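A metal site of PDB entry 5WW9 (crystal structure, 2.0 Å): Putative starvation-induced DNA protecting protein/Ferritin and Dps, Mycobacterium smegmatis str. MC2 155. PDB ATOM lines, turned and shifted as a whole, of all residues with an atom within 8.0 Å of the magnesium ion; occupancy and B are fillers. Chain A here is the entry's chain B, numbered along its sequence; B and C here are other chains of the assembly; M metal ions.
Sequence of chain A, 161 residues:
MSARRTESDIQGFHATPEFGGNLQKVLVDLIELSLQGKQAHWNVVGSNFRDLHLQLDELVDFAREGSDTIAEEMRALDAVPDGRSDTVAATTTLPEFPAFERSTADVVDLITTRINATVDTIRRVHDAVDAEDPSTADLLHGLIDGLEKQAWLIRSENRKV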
ATOM      1  N   SER A  47      30.268 -18.247  -8.459  1.00  0.00           N
ATOM      2  CA  SER A  47      29.018 -18.718  -9.062  1.00  0.00           C
ATOM      3  C   SER A  47      28.783 -20.185  -8.777  1.00  0.00           C
ATOM      4  O   SER A  47      29.624 -21.027  -9.085  1.00  0.00           O
ATOM      5  CB  SER A  47      29.036 -18.482 -10.583  1.00  0.00           C
ATOM      6  OG  SER A  47      29.056 -17.100 -10.874  1.00  0.00           O
ATOM      7  N   ASN A  48      27.621 -20.476  -8.206  1.00  0.00           N
ATOM      8  CA  ASN A  48      27.231 -21.819  -7.789  1.00  0.00           C
ATOM      9  C   ASN A  48      28.119 -22.408  -6.689  1.00  0.00           C
ATOM     10  O   ASN A  48      28.344 -23.619  -6.647  1.00  0.00           O
ATOM     11  CB  ASN A  48      27.075 -22.776  -8.983  1.00  0.00           C
ATOM     12  CG  ASN A  48      26.139 -23.912  -8.666  1.00  0.00           C
ATOM     13  OD1 ASN A  48      25.242 -23.759  -7.833  1.00  0.00           O
ATOM     14  ND2 ASN A  48      26.347 -25.049  -9.303  1.00  0.00           N
ATOM     15  N   PHE A  49      28.595 -21.533  -5.804  1.00  0.00           N
ATOM     16  CA  PHE A  49      29.324 -21.939  -4.602  1.00  0.00           C
ATOM     17  C   PHE A  49      28.691 -23.107  -3.843  1.00  0.00           C
ATOM     18  O   PHE A  49      29.363 -24.100  -3.543  1.00  0.00           O
ATOM     19  CB  PHE A  49      29.476 -20.742  -3.650  1.00  0.00           C
ATOM     20  CG  PHE A  49      29.800 -21.127  -2.237  1.00  0.00           C
ATOM     21  CD1 PHE A  49      31.096 -21.494  -1.873  1.00  0.00           C
ATOM     22  CD2 PHE A  49      28.802 -21.136  -1.260  1.00  0.00           C
ATOM     23  CE1 PHE A  49      31.395 -21.855  -0.568  1.00  0.00           C
ATOM     24  CE2 PHE A  49      29.085 -21.502   0.048  1.00  0.00           C
ATOM     25  CZ  PHE A  49      30.385 -21.857   0.391  1.00  0.00           C
ATOM     26  N   ARG A  50      27.402 -22.965  -3.508  1.00  0.00           N
ATOM     27  CA  ARG A  50      26.741 -23.863  -2.560  1.00  0.00           C
ATOM     28  C   ARG A  50      26.740 -25.302  -3.053  1.00  0.00           C
ATOM     29  O   ARG A  50      27.138 -26.199  -2.295  1.00  0.00           O
ATOM     30  CB  ARG A  50      25.340 -23.371  -2.216  1.00  0.00           C
ATOM     31  CG  ARG A  50      24.649 -24.217  -1.153  1.00  0.00           C
ATOM     32  CD  ARG A  50      23.334 -23.608  -0.727  1.00  0.00           C
ATOM     33  NE  ARG A  50      22.655 -24.428   0.272  1.00  0.00           N
ATOM     34  CZ  ARG A  50      21.847 -25.453  -0.004  1.00  0.00           C
ATOM     35  NH1 ARG A  50      21.605 -25.809  -1.256  1.00  0.00           N
ATOM     36  NH2 ARG A  50      21.279 -26.123   0.996  1.00  0.00           N
ATOM     37  N   ASP A  51      26.315 -25.518  -4.305  1.00  0.00           N
ATOM     38  CA  ASP A  51      26.330 -26.837  -4.938  1.00  0.00           C
ATOM     39  C   ASP A  51      27.695 -27.510  -4.861  1.00  0.00           C
ATOM     40  O   ASP A  51      27.789 -28.701  -4.561  1.00  0.00           O
ATOM     41  CB  ASP A  51      25.906 -26.763  -6.399  1.00  0.00           C
ATOM     42  CG  ASP A  51      24.411 -26.978  -6.610  1.00  0.00           C
ATOM     43  OD1 ASP A  51      23.772 -27.757  -5.879  1.00  0.00           O
ATOM     44  OD2 ASP A  51      23.877 -26.352  -7.532  1.00  0.00           O
ATOM     45  N   LEU A  52      28.749 -26.752  -5.159  1.00  0.00           N
ATOM     46  CA  LEU A  52      30.088 -27.317  -5.164  1.00  0.00           C
ATOM     47  C   LEU A  52      30.592 -27.589  -3.767  1.00  0.00           C
ATOM     48  O   LEU A  52      31.138 -28.666  -3.516  1.00  0.00           O
ATOM     49  CB  LEU A  52      31.074 -26.444  -5.954  1.00  0.00           C
ATOM     50  CG  LEU A  52      31.259 -26.874  -7.413  1.00  0.00           C
ATOM     51  CD1 LEU A  52      31.786 -28.311  -7.516  1.00  0.00           C
ATOM     52  CD2 LEU A  52      29.986 -26.730  -8.235  1.00  0.00           C
ATOM     53  N   GLU A 157      29.361 -29.235 -14.167  1.00  0.00           N
ATOM     54  CA  GLU A 157      29.272 -27.785 -13.964  1.00  0.00           C
ATOM     55  C   GLU A 157      29.958 -26.944 -15.064  1.00  0.00           C
ATOM     56  O   GLU A 157      29.414 -25.911 -15.481  1.00  0.00           O
ATOM     57  CB  GLU A 157      29.835 -27.428 -12.571  1.00  0.00           C
ATOM     58  CG  GLU A 157      29.966 -25.944 -12.240  1.00  0.00           C
ATOM     59  CD  GLU A 157      28.658 -25.168 -12.283  1.00  0.00           C
ATOM     60  OE1 GLU A 157      28.702 -23.974 -12.623  1.00  0.00           O
ATOM     61  OE2 GLU A 157      27.591 -25.736 -11.977  1.00  0.00           O
ATOM     62  N   SER B  47      19.838 -16.886 -11.815  1.00  0.00           N
ATOM     63  CA  SER B  47      20.971 -17.816 -11.796  1.00  0.00           C
ATOM     64  C   SER B  47      21.211 -18.371 -10.401  1.00  0.00           C
ATOM     65  O   SER B  47      21.364 -17.623  -9.440  1.00  0.00           O
ATOM     66  CB  SER B  47      22.234 -17.134 -12.338  1.00  0.00           C
ATOM     67  OG  SER B  47      22.105 -16.845 -13.715  1.00  0.00           O
ATOM     68  N   ASN B  48      21.239 -19.702 -10.318  1.00  0.00           N
ATOM     69  CA  ASN B  48      21.431 -20.438  -9.058  1.00  0.00           C
ATOM     70  C   ASN B  48      20.327 -20.194  -8.014  1.00  0.00           C
ATOM     71  O   ASN B  48      20.576 -20.218  -6.790  1.00  0.00           O
ATOM     72  CB  ASN B  48      22.837 -20.211  -8.496  1.00  0.00           C
ATOM     73  CG  ASN B  48      23.284 -21.315  -7.565  1.00  0.00           C
ATOM     74  OD1 ASN B  48      22.827 -22.450  -7.695  1.00  0.00           O
ATOM     75  ND2 ASN B  48      24.143 -20.989  -6.614  1.00  0.00           N
ATOM     76  N   PHE B  49      19.099 -19.980  -8.510  1.00  0.00           N
ATOM     77  CA  PHE B  49      17.883 -19.846  -7.688  1.00  0.00           C
ATOM     78  C   PHE B  49      17.778 -20.898  -6.571  1.00  0.00           C
ATOM     79  O   PHE B  49      17.560 -20.557  -5.408  1.00  0.00           O
ATOM     80  CB  PHE B  49      16.620 -19.915  -8.575  1.00  0.00           C
ATOM     81  CG  PHE B  49      15.356 -20.275  -7.825  1.00  0.00           C
ATOM     82  CD1 PHE B  49      14.665 -19.311  -7.092  1.00  0.00           C
ATOM     83  CD2 PHE B  49      14.852 -21.577  -7.862  1.00  0.00           C
ATOM     84  CE1 PHE B  49      13.518 -19.637  -6.384  1.00  0.00           C
ATOM     85  CE2 PHE B  49      13.705 -21.913  -7.164  1.00  0.00           C
ATOM     86  CZ  PHE B  49      13.039 -20.948  -6.430  1.00  0.00           C
ATOM     87  N   ARG B  50      17.909 -22.167  -6.952  1.00  0.00           N
ATOM     88  CA  ARG B  50      17.560 -23.273  -6.066  1.00  0.00           C
ATOM     89  C   ARG B  50      18.463 -23.308  -4.828  1.00  0.00           C
ATOM     90  O   ARG B  50      17.965 -23.444  -3.715  1.00  0.00           O
ATOM     91  CB  ARG B  50      17.593 -24.617  -6.813  1.00  0.00           C
ATOM     92  CG  ARG B  50      17.074 -25.785  -5.991  1.00  0.00           C
ATOM     93  CD  ARG B  50      17.125 -27.066  -6.779  1.00  0.00           C
ATOM     94  NE  ARG B  50      16.692 -28.203  -5.970  1.00  0.00           N
ATOM     95  CZ  ARG B  50      17.483 -28.958  -5.205  1.00  0.00           C
ATOM     96  NH1 ARG B  50      18.790 -28.715  -5.122  1.00  0.00           N
ATOM     97  NH2 ARG B  50      16.963 -29.966  -4.525  1.00  0.00           N
ATOM     98  N   ASP B  51      19.769 -23.145  -5.045  1.00  0.00           N
ATOM     99  CA  ASP B  51      20.733 -23.079  -3.932  1.00  0.00           C
ATOM    100  C   ASP B  51      20.384 -21.963  -2.947  1.00  0.00           C
ATOM    101  O   ASP B  51      20.398 -22.204  -1.740  1.00  0.00           O
ATOM    102  CB  ASP B  51      22.143 -22.843  -4.454  1.00  0.00           C
ATOM    103  CG  ASP B  51      22.936 -24.123  -4.599  1.00  0.00           C
ATOM    104  OD1 ASP B  51      22.759 -25.079  -3.816  1.00  0.00           O
ATOM    105  OD2 ASP B  51      23.787 -24.159  -5.514  1.00  0.00           O
ATOM    106  N   LEU B  52      20.061 -20.780  -3.464  1.00  0.00           N
ATOM    107  CA  LEU B  52      19.745 -19.640  -2.601  1.00  0.00           C
ATOM    108  C   LEU B  52      18.406 -19.776  -1.901  1.00  0.00           C
ATOM    109  O   LEU B  52      18.307 -19.543  -0.708  1.00  0.00           O
ATOM    110  CB  LEU B  52      19.903 -18.293  -3.305  1.00  0.00           C
ATOM    111  CG  LEU B  52      21.286 -17.625  -3.209  1.00  0.00           C
ATOM    112  CD1 LEU B  52      21.674 -17.322  -1.757  1.00  0.00           C
ATOM    113  CD2 LEU B  52      22.373 -18.428  -3.923  1.00  0.00           C
ATOM    114  N   GLU B 157      28.517 -16.854  -2.997  1.00  0.00           N
ATOM    115  CA  GLU B 157      27.947 -16.866  -4.347  1.00  0.00           C
ATOM    116  C   GLU B 157      28.456 -15.688  -5.209  1.00  0.00           C
ATOM    117  O   GLU B 157      28.750 -15.872  -6.391  1.00  0.00           O
ATOM    118  CB  GLU B 157      26.397 -16.867  -4.266  1.00  0.00           C
ATOM    119  CG  GLU B 157      25.619 -16.666  -5.577  1.00  0.00           C
ATOM    120  CD  GLU B 157      25.828 -17.772  -6.616  1.00  0.00           C
ATOM    121  OE1 GLU B 157      25.779 -17.442  -7.816  1.00  0.00           O
ATOM    122  OE2 GLU B 157      26.032 -18.951  -6.256  1.00  0.00           O
ATOM    123  N   SER C  47      26.305 -24.770 -16.357  1.00  0.00           N
ATOM    124  CA  SER C  47      26.112 -23.894 -15.197  1.00  0.00           C
ATOM    125  C   SER C  47      24.919 -24.318 -14.344  1.00  0.00           C
ATOM    126  O   SER C  47      23.800 -24.434 -14.829  1.00  0.00           O
ATOM    127  CB  SER C  47      25.956 -22.420 -15.627  1.00  0.00           C
ATOM    128  OG  SER C  47      27.129 -21.971 -16.275  1.00  0.00           O
ATOM    129  N   ASN C  48      25.197 -24.547 -13.062  1.00  0.00           N
ATOM    130  CA  ASN C  48      24.203 -25.008 -12.064  1.00  0.00           C
ATOM    131  C   ASN C  48      23.628 -26.402 -12.337  1.00  0.00           C
ATOM    132  O   ASN C  48      22.453 -26.663 -12.039  1.00  0.00           O
ATOM    133  CB  ASN C  48      23.081 -23.963 -11.837  1.00  0.00           C
ATOM    134  CG  ASN C  48      22.453 -24.079 -10.465  1.00  0.00           C
ATOM    135  OD1 ASN C  48      23.103 -24.506  -9.511  1.00  0.00           O
ATOM    136  ND2 ASN C  48      21.198 -23.684 -10.341  1.00  0.00           N
ATOM    137  N   PHE C  49      24.471 -27.278 -12.892  1.00  0.00           N
ATOM    138  CA  PHE C  49      24.157 -28.697 -13.135  1.00  0.00           C
ATOM    139  C   PHE C  49      23.499 -29.369 -11.921  1.00  0.00           C
ATOM    140  O   PHE C  49      22.404 -29.934 -12.053  1.00  0.00           O
ATOM    141  CB  PHE C  49      25.441 -29.471 -13.539  1.00  0.00           C
ATOM    142  CG  PHE C  49      25.326 -30.961 -13.369  1.00  0.00           C
ATOM    143  CD1 PHE C  49      25.913 -31.600 -12.269  1.00  0.00           C
ATOM    144  CD2 PHE C  49      24.623 -31.736 -14.296  1.00  0.00           C
ATOM    145  CE1 PHE C  49      25.792 -32.978 -12.102  1.00  0.00           C
ATOM    146  CE2 PHE C  49      24.502 -33.115 -14.129  1.00  0.00           C
ATOM    147  CZ  PHE C  49      25.089 -33.731 -13.031  1.00  0.00           C
ATOM    148  N   ARG C  50      24.165 -29.305 -10.776  1.00  0.00           N
ATOM    149  CA  ARG C  50      23.775 -30.094  -9.599  1.00  0.00           C
ATOM    150  C   ARG C  50      22.360 -29.790  -9.108  1.00  0.00           C
ATOM    151  O   ARG C  50      21.580 -30.721  -8.862  1.00  0.00           O
ATOM    152  CB  ARG C  50      24.797 -29.924  -8.476  1.00  0.00           C
ATOM    153  CG  ARG C  50      24.553 -30.840  -7.288  1.00  0.00           C
ATOM    154  CD  ARG C  50      25.637 -30.618  -6.250  1.00  0.00           C
ATOM    155  NE  ARG C  50      25.448 -31.498  -5.104  1.00  0.00           N
ATOM    156  CZ  ARG C  50      24.699 -31.229  -4.041  1.00  0.00           C
ATOM    157  NH1 ARG C  50      24.023 -30.078  -3.946  1.00  0.00           N
ATOM    158  NH2 ARG C  50      24.636 -32.118  -3.054  1.00  0.00           N
ATOM    159  N   ASP C  51      22.035 -28.505  -8.984  1.00  0.00           N
ATOM    160  CA  ASP C  51      20.702 -28.071  -8.586  1.00  0.00           C
ATOM    161  C   ASP C  51      19.627 -28.664  -9.481  1.00  0.00           C
ATOM    162  O   ASP C  51      18.657 -29.221  -8.986  1.00  0.00           O
ATOM    163  CB  ASP C  51      20.601 -26.537  -8.569  1.00  0.00           C
ATOM    164  CG  ASP C  51      20.841 -25.944  -7.202  1.00  0.00           C
ATOM    165  OD1 ASP C  51      20.455 -26.551  -6.179  1.00  0.00           O
ATOM    166  OD2 ASP C  51      21.406 -24.833  -7.148  1.00  0.00           O
ATOM    167  N   LEU C  52      19.826 -28.562 -10.799  1.00  0.00           N
ATOM    168  CA  LEU C  52      18.822 -29.037 -11.736  1.00  0.00           C
ATOM    169  C   LEU C  52      18.764 -30.547 -11.763  1.00  0.00           C
ATOM    170  O   LEU C  52      17.673 -31.122 -11.743  1.00  0.00           O
ATOM    171  CB  LEU C  52      19.012 -28.440 -13.140  1.00  0.00           C
ATOM    172  CG  LEU C  52      18.202 -27.163 -13.417  1.00  0.00           C
ATOM    173  CD1 LEU C  52      16.704 -27.450 -13.235  1.00  0.00           C
ATOM    174  CD2 LEU C  52      18.664 -26.007 -12.554  1.00  0.00           C
ATOM    175  N   GLU C 157      15.271 -20.555 -12.393  1.00  0.00           N
ATOM    176  CA  GLU C 157      16.678 -20.560 -12.814  1.00  0.00           C
ATOM    177  C   GLU C 157      16.956 -19.635 -14.007  1.00  0.00           C
ATOM    178  O   GLU C 157      17.992 -18.958 -14.043  1.00  0.00           O
ATOM    179  CB  GLU C 157      17.119 -22.010 -13.122  1.00  0.00           C
ATOM    180  CG  GLU C 157      18.523 -22.151 -13.738  1.00  0.00           C
ATOM    181  CD  GLU C 157      19.642 -21.583 -12.873  1.00  0.00           C
ATOM    182  OE1 GLU C 157      19.584 -21.713 -11.624  1.00  0.00           O
ATOM    183  OE2 GLU C 157      20.593 -21.020 -13.437  1.00  0.00           O
HETATM  184 MG    MG M   1      23.366 -24.294  -7.559  1.00  0.00          MG
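The side-chain amide nitrogen of Asn 48 of chain B is in hydrogen-bond range of the side-chain carboxylate of Glu 157 of chain B, at 2.8 Å. The side-chain carboxylate of Glu 157 of chain C is in hydrogen-bond range of the backbone NH of Asn 48 of chain B, 2.9 Å away. N of Asn 48 of chain A is in hydrogen-bond range of OE2 of Glu 157 of chain B (2.9 Å). The side-chain carboxylate (OE2) of Glu 157 of chain A is in hydrogen-bond range of the side-chain amide nitrogen (ND2) of Asn 48 of chain A (3.0 Å). ND2 of Asn 48 of chain C sits at hydrogen-bond distance from OE1 of Glu 157 of chain C (2.9 Å). N of Asn 48 of chain C is in hydrogen-bond range of OE2 of Glu 157 of chain A (2.9 Å). NH1 of Arg 50 of chain B lies within salt-bridge range of OD1 of Asp 51 of chain C. The side-chain carboxylate (OD1) of Asp 51 of chain B is in salt-bridge range of the guanidinium group (NH1) of Arg 50 of chain A, at 2.9 Å.
Six residues have an atom within 4 Å of the magnesium ion: Asn 48 of chain A, Asp 51 of chain A, Asn 48 of chain B, Asp 51 of chain B, Asn 48 of chain C and Asp 51 of chain C. The nearest printed residue that does not touch the magnesium ion is Arg 50 of chain B (5.7 Å).
The magnesium ion is bound by OD1 of Asn 48 of chain B (1.9 Å), OD1 of Asn 48 of chain A (2.0 Å), OD1 of Asn 48 of chain C (2.0 Å), OD2 of Asp 51 of chain C (2.1 Å), OD2 of Asp 51 of chain B (2.1 Å) and OD2 of Asp 51 of chain A (2.1 Å).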
